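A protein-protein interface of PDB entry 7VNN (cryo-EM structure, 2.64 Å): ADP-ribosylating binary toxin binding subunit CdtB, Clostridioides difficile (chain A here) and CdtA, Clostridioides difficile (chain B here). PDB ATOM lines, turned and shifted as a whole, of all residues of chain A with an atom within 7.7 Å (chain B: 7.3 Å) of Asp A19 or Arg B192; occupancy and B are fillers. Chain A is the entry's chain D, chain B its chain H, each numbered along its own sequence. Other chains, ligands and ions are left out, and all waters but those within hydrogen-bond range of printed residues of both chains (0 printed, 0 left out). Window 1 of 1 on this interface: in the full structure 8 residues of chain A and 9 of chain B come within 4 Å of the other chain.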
ATOM      1  N   TRP A  13      -1.156  20.673  27.593  1.00  0.00           N
ATOM      2  CA  TRP A  13      -1.031  21.971  28.247  1.00  0.00           C
ATOM      3  C   TRP A  13      -1.747  23.094  27.499  1.00  0.00           C
ATOM      4  O   TRP A  13      -2.042  22.987  26.311  1.00  0.00           O
ATOM      5  CB  TRP A  13       0.446  22.310  28.459  1.00  0.00           C
ATOM      6  CG  TRP A  13       1.342  21.948  27.318  1.00  0.00           C
ATOM      7  CD1 TRP A  13       1.972  20.755  27.131  1.00  0.00           C
ATOM      8  CD2 TRP A  13       1.731  22.782  26.223  1.00  0.00           C
ATOM      9  NE1 TRP A  13       2.722  20.787  25.983  1.00  0.00           N
ATOM     10  CE2 TRP A  13       2.593  22.021  25.406  1.00  0.00           C
ATOM     11  CE3 TRP A  13       1.431  24.093  25.846  1.00  0.00           C
ATOM     12  CZ2 TRP A  13       3.156  22.528  24.240  1.00  0.00           C
ATOM     13  CZ3 TRP A  13       1.996  24.595  24.691  1.00  0.00           C
ATOM     14  CH2 TRP A  13       2.847  23.814  23.902  1.00  0.00           C
ATOM     15  N   GLU A  16      -2.679  26.334  21.912  1.00  0.00           N
ATOM     16  CA  GLU A  16      -3.275  25.805  20.685  1.00  0.00           C
ATOM     17  C   GLU A  16      -2.235  25.243  19.726  1.00  0.00           C
ATOM     18  O   GLU A  16      -2.367  25.380  18.507  1.00  0.00           O
ATOM     19  CB  GLU A  16      -4.101  26.884  19.995  1.00  0.00           C
ATOM     20  CG  GLU A  16      -5.161  27.520  20.874  1.00  0.00           C
ATOM     21  CD  GLU A  16      -6.323  26.589  21.149  1.00  0.00           C
ATOM     22  OE1 GLU A  16      -6.190  25.713  22.029  1.00  0.00           O
ATOM     23  OE2 GLU A  16      -7.369  26.731  20.481  1.00  0.00           O
ATOM     24  N   ASP A  17      -1.184  24.618  20.246  1.00  0.00           N
ATOM     25  CA  ASP A  17      -0.128  24.024  19.433  1.00  0.00           C
ATOM     26  C   ASP A  17       0.250  22.643  19.964  1.00  0.00           C
ATOM     27  O   ASP A  17       1.425  22.309  20.134  1.00  0.00           O
ATOM     28  CB  ASP A  17       1.072  24.965  19.353  1.00  0.00           C
ATOM     29  CG  ASP A  17       1.652  25.291  20.713  1.00  0.00           C
ATOM     30  OD1 ASP A  17       1.086  24.837  21.726  1.00  0.00           O
ATOM     31  OD2 ASP A  17       2.673  26.008  20.766  1.00  0.00           O
ATOM     32  N   LEU A  18      -0.758  21.819  20.240  1.00  0.00           N
ATOM     33  CA  LEU A  18      -0.564  20.434  20.648  1.00  0.00           C
ATOM     34  C   LEU A  18      -1.011  19.514  19.522  1.00  0.00           C
ATOM     35  O   LEU A  18      -2.096  19.697  18.960  1.00  0.00           O
ATOM     36  CB  LEU A  18      -1.340  20.115  21.924  1.00  0.00           C
ATOM     37  CG  LEU A  18      -0.731  20.579  23.241  1.00  0.00           C
ATOM     38  CD1 LEU A  18      -1.796  20.576  24.312  1.00  0.00           C
ATOM     39  CD2 LEU A  18       0.424  19.675  23.632  1.00  0.00           C
ATOM     40  N   ASP A  19      -0.179  18.524  19.206  1.00  0.00           N
ATOM     41  CA  ASP A  19      -0.398  17.616  18.081  1.00  0.00           C
ATOM     42  C   ASP A  19      -0.152  16.176  18.536  1.00  0.00           C
ATOM     43  O   ASP A  19       0.658  15.452  17.963  1.00  0.00           O
ATOM     44  CB  ASP A  19       0.482  17.983  16.891  1.00  0.00           C
ATOM     45  CG  ASP A  19      -0.071  17.462  15.583  1.00  0.00           C
ATOM     46  OD1 ASP A  19      -1.155  16.845  15.601  1.00  0.00           O
ATOM     47  OD2 ASP A  19       0.576  17.668  14.536  1.00  0.00           O
ATOM     48  N   THR A  20      -0.845  15.779  19.608  1.00  0.00           N
ATOM     49  CA  THR A  20      -0.553  14.523  20.298  1.00  0.00           C
ATOM     50  C   THR A  20      -0.472  13.334  19.345  1.00  0.00           C
ATOM     51  O   THR A  20       0.410  12.480  19.485  1.00  0.00           O
ATOM     52  CB  THR A  20      -1.613  14.261  21.367  1.00  0.00           C
ATOM     53  OG1 THR A  20      -1.890  15.476  22.074  1.00  0.00           O
ATOM     54  CG2 THR A  20      -1.130  13.213  22.352  1.00  0.00           C
ATOM     55  N   ASP A  21      -1.378  13.255  18.374  1.00  0.00           N
ATOM     56  CA  ASP A  21      -1.353  12.163  17.408  1.00  0.00           C
ATOM     57  C   ASP A  21      -0.448  12.444  16.218  1.00  0.00           C
ATOM     58  O   ASP A  21      -0.232  11.544  15.399  1.00  0.00           O
ATOM     59  CB  ASP A  21      -2.768  11.852  16.916  1.00  0.00           C
ATOM     60  CG  ASP A  21      -3.483  13.072  16.396  1.00  0.00           C
ATOM     61  OD1 ASP A  21      -2.901  14.172  16.457  1.00  0.00           O
ATOM     62  OD2 ASP A  21      -4.629  12.932  15.925  1.00  0.00           O
ATOM     63  N   ASN A  22       0.077  13.665  16.104  1.00  0.00           N
ATOM     64  CA  ASN A  22       1.057  14.031  15.080  1.00  0.00           C
ATOM     65  C   ASN A  22       0.493  13.835  13.669  1.00  0.00           C
ATOM     66  O   ASN A  22       0.996  13.047  12.867  1.00  0.00           O
ATOM     67  CB  ASN A  22       2.359  13.245  15.278  1.00  0.00           C
ATOM     68  CG  ASN A  22       3.491  13.769  14.424  1.00  0.00           C
ATOM     69  OD1 ASN A  22       3.572  14.962  14.147  1.00  0.00           O
ATOM     70  ND2 ASN A  22       4.379  12.876  14.007  1.00  0.00           N
ATOM     71  N   ASP A  23      -0.579  14.580  13.377  1.00  0.00           N
ATOM     72  CA  ASP A  23      -1.199  14.551  12.056  1.00  0.00           C
ATOM     73  C   ASP A  23      -1.441  15.953  11.504  1.00  0.00           C
ATOM     74  O   ASP A  23      -2.316  16.134  10.653  1.00  0.00           O
ATOM     75  CB  ASP A  23      -2.506  13.754  12.082  1.00  0.00           C
ATOM     76  CG  ASP A  23      -3.564  14.386  12.964  1.00  0.00           C
ATOM     77  OD1 ASP A  23      -3.214  15.220  13.822  1.00  0.00           O
ATOM     78  OD2 ASP A  23      -4.751  14.041  12.800  1.00  0.00           O
ATOM     79  N   ASN A  24      -0.686  16.945  11.977  1.00  0.00           N
ATOM     80  CA  ASN A  24      -0.680  18.322  11.489  1.00  0.00           C
ATOM     81  C   ASN A  24      -1.982  19.070  11.748  1.00  0.00           C
ATOM     82  O   ASN A  24      -2.247  20.077  11.081  1.00  0.00           O
ATOM     83  CB  ASN A  24      -0.347  18.396   9.995  1.00  0.00           C
ATOM     84  CG  ASN A  24       0.972  17.735   9.661  1.00  0.00           C
ATOM     85  OD1 ASN A  24       1.977  17.951  10.339  1.00  0.00           O
ATOM     86  ND2 ASN A  24       0.976  16.918   8.613  1.00  0.00           N
ATOM     87  N   ILE A  25      -2.802  18.615  12.688  1.00  0.00           N
ATOM     88  CA  ILE A  25      -4.000  19.326  13.115  1.00  0.00           C
ATOM     89  C   ILE A  25      -3.939  19.465  14.629  1.00  0.00           C
ATOM     90  O   ILE A  25      -3.814  18.458  15.326  1.00  0.00           O
ATOM     91  CB  ILE A  25      -5.298  18.611  12.696  1.00  0.00           C
ATOM     92  CG1 ILE A  25      -5.209  18.128  11.249  1.00  0.00           C
ATOM     93  CG2 ILE A  25      -6.484  19.542  12.854  1.00  0.00           C
ATOM     94  CD1 ILE A  25      -6.295  17.153  10.873  1.00  0.00           C
ATOM     95  N   PRO A  26      -4.011  20.676  15.177  1.00  0.00           N
ATOM     96  CA  PRO A  26      -3.963  20.833  16.634  1.00  0.00           C
ATOM     97  C   PRO A  26      -5.145  20.165  17.320  1.00  0.00           C
ATOM     98  O   PRO A  26      -6.199  19.932  16.725  1.00  0.00           O
ATOM     99  CB  PRO A  26      -3.992  22.353  16.829  1.00  0.00           C
ATOM    100  CG  PRO A  26      -3.464  22.904  15.553  1.00  0.00           C
ATOM    101  CD  PRO A  26      -3.922  21.968  14.477  1.00  0.00           C
ATOM    102  N   ASP A  27      -4.945  19.846  18.602  1.00  0.00           N
ATOM    103  CA  ASP A  27      -5.969  19.147  19.375  1.00  0.00           C
ATOM    104  C   ASP A  27      -7.242  19.973  19.503  1.00  0.00           C
ATOM    105  O   ASP A  27      -8.351  19.437  19.390  1.00  0.00           O
ATOM    106  CB  ASP A  27      -5.429  18.800  20.761  1.00  0.00           C
ATOM    107  CG  ASP A  27      -4.306  17.793  20.713  1.00  0.00           C
ATOM    108  OD1 ASP A  27      -4.149  17.131  19.666  1.00  0.00           O
ATOM    109  OD2 ASP A  27      -3.584  17.657  21.722  1.00  0.00           O
ATOM    110  N   SER A  28      -7.102  21.276  19.757  1.00  0.00           N
ATOM    111  CA  SER A  28      -8.273  22.125  19.949  1.00  0.00           C
ATOM    112  C   SER A  28      -9.125  22.185  18.689  1.00  0.00           C
ATOM    113  O   SER A  28     -10.360  22.156  18.763  1.00  0.00           O
ATOM    114  CB  SER A  28      -7.839  23.526  20.369  1.00  0.00           C
ATOM    115  OG  SER A  28      -7.195  23.499  21.629  1.00  0.00           O
ATOM    116  N   GLU A  30      -9.378  19.875  16.362  1.00  0.00           N
ATOM    117  CA  GLU A  30     -10.047  18.591  16.196  1.00  0.00           C
ATOM    118  C   GLU A  30     -11.198  18.423  17.177  1.00  0.00           C
ATOM    119  O   GLU A  30     -12.223  17.827  16.828  1.00  0.00           O
ATOM    120  CB  GLU A  30      -9.044  17.449  16.361  1.00  0.00           C
ATOM    121  CG  GLU A  30      -8.082  17.311  15.200  1.00  0.00           C
ATOM    122  CD  GLU A  30      -7.312  16.012  15.227  1.00  0.00           C
ATOM    123  OE1 GLU A  30      -7.820  15.009  14.689  1.00  0.00           O
ATOM    124  OE2 GLU A  30      -6.196  15.991  15.783  1.00  0.00           O
ATOM    125  N   TYR A  60      -8.569  13.318  18.324  1.00  0.00           N
ATOM    126  CA  TYR A  60      -7.282  13.981  18.486  1.00  0.00           C
ATOM    127  C   TYR A  60      -6.210  13.069  19.065  1.00  0.00           C
ATOM    128  O   TYR A  60      -5.061  13.501  19.207  1.00  0.00           O
ATOM    129  CB  TYR A  60      -7.435  15.233  19.359  1.00  0.00           C
ATOM    130  CG  TYR A  60      -7.563  14.966  20.840  1.00  0.00           C
ATOM    131  CD1 TYR A  60      -8.793  14.667  21.407  1.00  0.00           C
ATOM    132  CD2 TYR A  60      -6.457  15.027  21.674  1.00  0.00           C
ATOM    133  CE1 TYR A  60      -8.914  14.428  22.761  1.00  0.00           C
ATOM    134  CE2 TYR A  60      -6.569  14.789  23.026  1.00  0.00           C
ATOM    135  CZ  TYR A  60      -7.798  14.491  23.564  1.00  0.00           C
ATOM    136  OH  TYR A  60      -7.910  14.254  24.912  1.00  0.00           O
ATOM    137  N   LEU A  61      -6.551  11.829  19.406  1.00  0.00           N
ATOM    138  CA  LEU A  61      -5.578  10.848  19.863  1.00  0.00           C
ATOM    139  C   LEU A  61      -5.318   9.758  18.835  1.00  0.00           C
ATOM    140  O   LEU A  61      -4.549   8.832  19.112  1.00  0.00           O
ATOM    141  CB  LEU A  61      -6.038  10.218  21.181  1.00  0.00           C
ATOM    142  CG  LEU A  61      -5.944  11.099  22.427  1.00  0.00           C
ATOM    143  CD1 LEU A  61      -6.234  10.288  23.674  1.00  0.00           C
ATOM    144  CD2 LEU A  61      -4.580  11.756  22.518  1.00  0.00           C
ATOM    145  N   GLU B 113       7.794  12.669  29.486  1.00  0.00           N
ATOM    146  CA  GLU B 113       7.073  13.889  29.161  1.00  0.00           C
ATOM    147  C   GLU B 113       7.965  15.112  29.327  1.00  0.00           C
ATOM    148  O   GLU B 113       8.924  15.104  30.105  1.00  0.00           O
ATOM    149  CB  GLU B 113       5.817  14.038  30.033  1.00  0.00           C
ATOM    150  CG  GLU B 113       6.085  14.481  31.458  1.00  0.00           C
ATOM    151  CD  GLU B 113       4.854  15.065  32.122  1.00  0.00           C
ATOM    152  OE1 GLU B 113       3.730  14.752  31.675  1.00  0.00           O
ATOM    153  OE2 GLU B 113       5.010  15.835  33.093  1.00  0.00           O
ATOM    154  N   ILE B 114       7.641  16.162  28.577  1.00  0.00           N
ATOM    155  CA  ILE B 114       8.364  17.426  28.626  1.00  0.00           C
ATOM    156  C   ILE B 114       7.496  18.456  29.332  1.00  0.00           C
ATOM    157  O   ILE B 114       6.262  18.412  29.271  1.00  0.00           O
ATOM    158  CB  ILE B 114       8.774  17.923  27.222  1.00  0.00           C
ATOM    159  CG1 ILE B 114       7.547  18.326  26.405  1.00  0.00           C
ATOM    160  CG2 ILE B 114       9.551  16.851  26.481  1.00  0.00           C
ATOM    161  CD1 ILE B 114       7.892  18.996  25.093  1.00  0.00           C
ATOM    162  N   SER B 115       8.154  19.385  30.018  1.00  0.00           N
ATOM    163  CA  SER B 115       7.454  20.413  30.772  1.00  0.00           C
ATOM    164  C   SER B 115       6.952  21.520  29.848  1.00  0.00           C
ATOM    165  O   SER B 115       7.517  21.789  28.786  1.00  0.00           O
ATOM    166  CB  SER B 115       8.368  21.001  31.848  1.00  0.00           C
ATOM    167  OG  SER B 115       7.870  22.239  32.324  1.00  0.00           O
ATOM    168  N   LEU B 116       5.861  22.161  30.273  1.00  0.00           N
ATOM    169  CA  LEU B 116       5.368  23.334  29.560  1.00  0.00           C
ATOM    170  C   LEU B 116       6.397  24.458  29.585  1.00  0.00           C
ATOM    171  O   LEU B 116       6.604  25.146  28.576  1.00  0.00           O
ATOM    172  CB  LEU B 116       4.045  23.794  30.173  1.00  0.00           C
ATOM    173  CG  LEU B 116       3.522  25.193  29.842  1.00  0.00           C
ATOM    174  CD1 LEU B 116       3.375  25.399  28.348  1.00  0.00           C
ATOM    175  CD2 LEU B 116       2.195  25.420  30.543  1.00  0.00           C
ATOM    176  N   PHE B 119       9.264  23.804  27.115  1.00  0.00           N
ATOM    177  CA  PHE B 119       8.740  24.139  25.796  1.00  0.00           C
ATOM    178  C   PHE B 119       8.740  25.647  25.578  1.00  0.00           C
ATOM    179  O   PHE B 119       9.062  26.122  24.485  1.00  0.00           O
ATOM    180  CB  PHE B 119       7.330  23.566  25.635  1.00  0.00           C
ATOM    181  CG  PHE B 119       6.800  23.630  24.230  1.00  0.00           C
ATOM    182  CD1 PHE B 119       6.244  24.797  23.733  1.00  0.00           C
ATOM    183  CD2 PHE B 119       6.847  22.518  23.408  1.00  0.00           C
ATOM    184  CE1 PHE B 119       5.757  24.857  22.440  1.00  0.00           C
ATOM    185  CE2 PHE B 119       6.357  22.570  22.116  1.00  0.00           C
ATOM    186  CZ  PHE B 119       5.810  23.740  21.632  1.00  0.00           C
ATOM    187  N   LYS B 189       7.599  27.025  13.458  1.00  0.00           N
ATOM    188  CA  LYS B 189       6.793  26.631  14.602  1.00  0.00           C
ATOM    189  C   LYS B 189       7.321  25.333  15.195  1.00  0.00           C
ATOM    190  O   LYS B 189       7.967  24.535  14.510  1.00  0.00           O
ATOM    191  CB  LYS B 189       5.315  26.459  14.216  1.00  0.00           C
ATOM    192  CG  LYS B 189       5.060  25.351  13.203  1.00  0.00           C
ATOM    193  CD  LYS B 189       3.597  25.304  12.790  1.00  0.00           C
ATOM    194  CE  LYS B 189       2.726  24.767  13.913  1.00  0.00           C
ATOM    195  NZ  LYS B 189       1.297  24.672  13.518  1.00  0.00           N
ATOM    196  N   ILE B 190       7.049  25.137  16.483  1.00  0.00           N
ATOM    197  CA  ILE B 190       7.372  23.902  17.184  1.00  0.00           C
ATOM    198  C   ILE B 190       6.134  23.443  17.942  1.00  0.00           C
ATOM    199  O   ILE B 190       5.389  24.263  18.490  1.00  0.00           O
ATOM    200  CB  ILE B 190       8.575  24.072  18.141  1.00  0.00           C
ATOM    201  CG1 ILE B 190       8.265  25.086  19.242  1.00  0.00           C
ATOM    202  CG2 ILE B 190       9.821  24.491  17.375  1.00  0.00           C
ATOM    203  CD1 ILE B 190       9.009  24.818  20.528  1.00  0.00           C
ATOM    204  N   VAL B 191       5.899  22.130  17.950  1.00  0.00           N
ATOM    205  CA  VAL B 191       4.759  21.534  18.635  1.00  0.00           C
ATOM    206  C   VAL B 191       5.236  20.307  19.403  1.00  0.00           C
ATOM    207  O   VAL B 191       6.345  19.811  19.204  1.00  0.00           O
ATOM    208  CB  VAL B 191       3.624  21.144  17.664  1.00  0.00           C
ATOM    209  CG1 VAL B 191       2.946  22.385  17.105  1.00  0.00           C
ATOM    210  CG2 VAL B 191       4.165  20.275  16.546  1.00  0.00           C
ATOM    211  N   ARG B 192       4.374  19.819  20.290  1.00  0.00           N
ATOM    212  CA  ARG B 192       4.633  18.613  21.064  1.00  0.00           C
ATOM    213  C   ARG B 192       3.851  17.453  20.467  1.00  0.00           C
ATOM    214  O   ARG B 192       2.652  17.581  20.197  1.00  0.00           O
ATOM    215  CB  ARG B 192       4.253  18.802  22.534  1.00  0.00           C
ATOM    216  CG  ARG B 192       4.871  17.764  23.455  1.00  0.00           C
ATOM    217  CD  ARG B 192       4.226  17.773  24.831  1.00  0.00           C
ATOM    218  NE  ARG B 192       2.885  17.201  24.804  1.00  0.00           N
ATOM    219  CZ  ARG B 192       2.045  17.216  25.829  1.00  0.00           C
ATOM    220  NH1 ARG B 192       2.385  17.740  26.994  1.00  0.00           N
ATOM    221  NH2 ARG B 192       0.834  16.685  25.683  1.00  0.00           N
ATOM    222  N   ILE B 193       4.533  16.325  20.264  1.00  0.00           N
ATOM    223  CA  ILE B 193       3.943  15.131  19.680  1.00  0.00           C
ATOM    224  C   ILE B 193       4.322  13.929  20.533  1.00  0.00           C
ATOM    225  O   ILE B 193       5.270  13.968  21.320  1.00  0.00           O
ATOM    226  CB  ILE B 193       4.393  14.914  18.219  1.00  0.00           C
ATOM    227  CG1 ILE B 193       5.919  14.890  18.136  1.00  0.00           C
ATOM    228  CG2 ILE B 193       3.828  15.998  17.320  1.00  0.00           C
ATOM    229  CD1 ILE B 193       6.453  14.603  16.758  1.00  0.00           C
ATOM    230  N   VAL B 194       3.563  12.849  20.367  1.00  0.00           N
ATOM    231  CA  VAL B 194       3.773  11.612  21.109  1.00  0.00           C
ATOM    232  C   VAL B 194       4.155  10.519  20.121  1.00  0.00           C
ATOM    233  O   VAL B 194       3.389  10.215  19.199  1.00  0.00           O
ATOM    234  CB  VAL B 194       2.522  11.207  21.909  1.00  0.00           C
ATOM    235  CG1 VAL B 194       2.649   9.776  22.405  1.00  0.00           C
ATOM    236  CG2 VAL B 194       2.303  12.160  23.066  1.00  0.00           C
ATOM    237  N   LYS B 198       6.220   8.557  24.280  1.00  0.00           N
ATOM    238  CA  LYS B 198       7.133   9.578  24.769  1.00  0.00           C
ATOM    239  C   LYS B 198       6.846  10.902  24.075  1.00  0.00           C
ATOM    240  O   LYS B 198       6.389  10.934  22.930  1.00  0.00           O
ATOM    241  CB  LYS B 198       8.594   9.179  24.539  1.00  0.00           C
ATOM    242  CG  LYS B 198       9.219   8.388  25.672  1.00  0.00           C
ATOM    243  CD  LYS B 198      10.708   8.189  25.439  1.00  0.00           C
ATOM    244  CE  LYS B 198      11.357   7.453  26.598  1.00  0.00           C
ATOM    245  NZ  LYS B 198      12.825   7.310  26.406  1.00  0.00           N
ATOM    246  N   HIS B 199       7.119  11.996  24.781  1.00  0.00           N
ATOM    247  CA  HIS B 199       6.889  13.332  24.253  1.00  0.00           C
ATOM    248  C   HIS B 199       8.099  13.781  23.445  1.00  0.00           C
ATOM    249  O   HIS B 199       9.242  13.620  23.885  1.00  0.00           O
ATOM    250  CB  HIS B 199       6.619  14.325  25.385  1.00  0.00           C
ATOM    251  CG  HIS B 199       5.231  14.249  25.939  1.00  0.00           C
ATOM    252  ND1 HIS B 199       4.827  14.984  27.032  1.00  0.00           N
ATOM    253  CD2 HIS B 199       4.158  13.518  25.560  1.00  0.00           C
ATOM    254  CE1 HIS B 199       3.562  14.713  27.298  1.00  0.00           C
ATOM    255  NE2 HIS B 199       3.132  13.827  26.418  1.00  0.00           N
ATOM    256  N   TYR B 200       7.846  14.340  22.265  1.00  0.00           N
ATOM    257  CA  TYR B 200       8.889  14.890  21.413  1.00  0.00           C
ATOM    258  C   TYR B 200       8.454  16.261  20.915  1.00  0.00           C
ATOM    259  O   TYR B 200       7.272  16.614  20.944  1.00  0.00           O
ATOM    260  CB  TYR B 200       9.202  13.967  20.225  1.00  0.00           C
ATOM    261  CG  TYR B 200       9.857  12.660  20.614  1.00  0.00           C
ATOM    262  CD1 TYR B 200       9.112  11.623  21.157  1.00  0.00           C
ATOM    263  CD2 TYR B 200      11.222  12.466  20.442  1.00  0.00           C
ATOM    264  CE1 TYR B 200       9.703  10.432  21.515  1.00  0.00           C
ATOM    265  CE2 TYR B 200      11.823  11.275  20.799  1.00  0.00           C
ATOM    266  CZ  TYR B 200      11.058  10.261  21.336  1.00  0.00           C
ATOM    267  OH  TYR B 200      11.646   9.070  21.698  1.00  0.00           O
ATOM    268  N   ILE B 201       9.430  17.040  20.455  1.00  0.00           N
ATOM    269  CA  ILE B 201       9.193  18.361  19.886  1.00  0.00           C
ATOM    270  C   ILE B 201       9.363  18.260  18.377  1.00  0.00           C
ATOM    271  O   ILE B 201      10.390  17.769  17.895  1.00  0.00           O
ATOM    272  CB  ILE B 201      10.143  19.413  20.485  1.00  0.00           C
ATOM    273  CG1 ILE B 201       9.645  19.854  21.863  1.00  0.00           C
ATOM    274  CG2 ILE B 201      10.272  20.612  19.559  1.00  0.00           C
ATOM    275  CD1 ILE B 201      10.483  20.939  22.503  1.00  0.00           C
ATOM    276  N   LYS B 202       8.354  18.709  17.637  1.00  0.00           N
ATOM    277  CA  LYS B 202       8.361  18.661  16.180  1.00  0.00           C
ATOM    278  C   LYS B 202       8.547  20.072  15.643  1.00  0.00           C
ATOM    279  O   LYS B 202       7.757  20.968  15.956  1.00  0.00           O
ATOM    280  CB  LYS B 202       7.068  18.048  15.642  1.00  0.00           C
ATOM    281  CG  LYS B 202       6.980  18.024  14.126  1.00  0.00           C
ATOM    282  CD  LYS B 202       5.776  17.229  13.653  1.00  0.00           C
ATOM    283  CE  LYS B 202       4.482  18.015  13.800  1.00  0.00           C
ATOM    284  NZ  LYS B 202       3.326  17.297  13.192  1.00  0.00           N
ATOM    285  N   GLU B 204       9.319  22.512  12.114  1.00  0.00           N
ATOM    286  CA  GLU B 204       9.322  22.643  10.663  1.00  0.00           C
ATOM    287  C   GLU B 204      10.315  23.728  10.269  1.00  0.00           C
ATOM    288  O   GLU B 204      10.254  24.849  10.787  1.00  0.00           O
ATOM    289  CB  GLU B 204       7.926  22.976  10.138  1.00  0.00           C
ATOM    290  CG  GLU B 204       7.024  21.764   9.959  1.00  0.00           C
ATOM    291  CD  GLU B 204       6.040  21.597  11.099  1.00  0.00           C
ATOM    292  OE1 GLU B 204       6.111  22.382  12.066  1.00  0.00           O
ATOM    293  OE2 GLU B 204       5.194  20.681  11.028  1.00  0.00           O
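N of Asp A19 lies within hydrogen-bond range of O of Arg B192, 3.1 Å away. The side-chain carboxylate of Asp A19 is in salt-bridge range of the side-chain amino group of Lys B202, at 3.1 Å. The backbone carbonyl oxygen (O) of Thr A20 lies within hydrogen-bond range of the backbone NH (N) of Val B194 (3.3 Å). The side-chain amide oxygen (OD1) of Asn A22 is in hydrogen-bond range of the side-chain amino group (NZ) of Lys B202 (2.5 Å). The side-chain amide oxygen (OD1) of Asn A24 lies within hydrogen-bond range of the side-chain amino group (NZ) of Lys B202, at 3.2 Å. The indole nitrogen of Trp A13 sits close to the guanidinium group of Arg B192 (3.2 Å).
O of Leu A18 lies within hydrogen-bond range of N of Asp A27, at 2.9 Å. The side-chain carboxylate of Asp A19 sits close to the backbone NH of Asn A22, at 3.4 Å. OD2 of Asp A19 lies within hydrogen-bond range of N of Asn A24, at 2.9 Å. OG1 of Thr A20 sits at hydrogen-bond distance from OD2 of Asp A27, at 2.8 Å. O of Val B191 is in hydrogen-bond range of N of Lys B202 (2.8 Å). The backbone carbonyl oxygen (O) of Ile B193 lies within hydrogen-bond range of the backbone NH (N) of Tyr B200, at 2.8 Å.
Among the printed residues, merely in contact across the chains: Trp A13 with Leu B116 (3.4 Å), Trp A13 with Phe B119 (3.4 Å), Asp A17 with Phe B119 (3.7 Å), Asp A17 with Ile B190 (3.9 Å), Asp A17 with Val B191 (3.4 Å), Asp A17 with Arg B192 (3.9 Å), Leu A18 with Arg B192 (3.6 Å), Asp A19 with Ile B193 (3.3 Å), Thr A20 with Arg B192 (3.98 Å) and Asn A22 with Ile B193 (3.3 Å).
Printed residues of chain B within 4 Å of Asp A17: Phe B119, Ile B190, Val B191 and Arg B192. Printed residues of chain B within 4 Å of Leu A18: Arg B192 (3.6 Å). Asp A19 touches just these residues of chain B: Arg B192 (3.1 Å), Ile B193 (3.3 Å) and Lys B202 (3.1 Å). Ile A25 touches none of the printed residues of chain B. Printed residues of chain A within 4 Å of Leu B116: Trp A13. Of chain A, only Trp A13 (3.0 Å), Asp A17 (3.9 Å), Leu A18 (3.6 Å), Asp A19 (3.1 Å) and Thr A20 (3.98 Å) come within 4 Å of Arg B192. Of the printed residues of chain A, Lys B202 touches Asp A19, Asn A22 and Asn A24. The nearest printed residue of chain A that does not touch Leu B116 is Asp A17 (7.0 Å).
Of the 17 printed residues of chain B, 8 touch a printed residue of chain A. Hydrophobic or aromatic side chains of chain B within 4 Å of the printed part of chain A: Leu B116, Phe B119, Val B191, Ile B193 and Val B194. Hydrophobic or aromatic side chains of chain A that line the printed part of chain B: Trp A13 and Leu A18. Among the printed residues, 16 pairs touch across the chains. Among the printed residues, Asp or Glu carboxylates within 4 Å of a Lys or Arg side-chain nitrogen of the other chain: Asp A19 with Lys B202 (3.1 Å).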
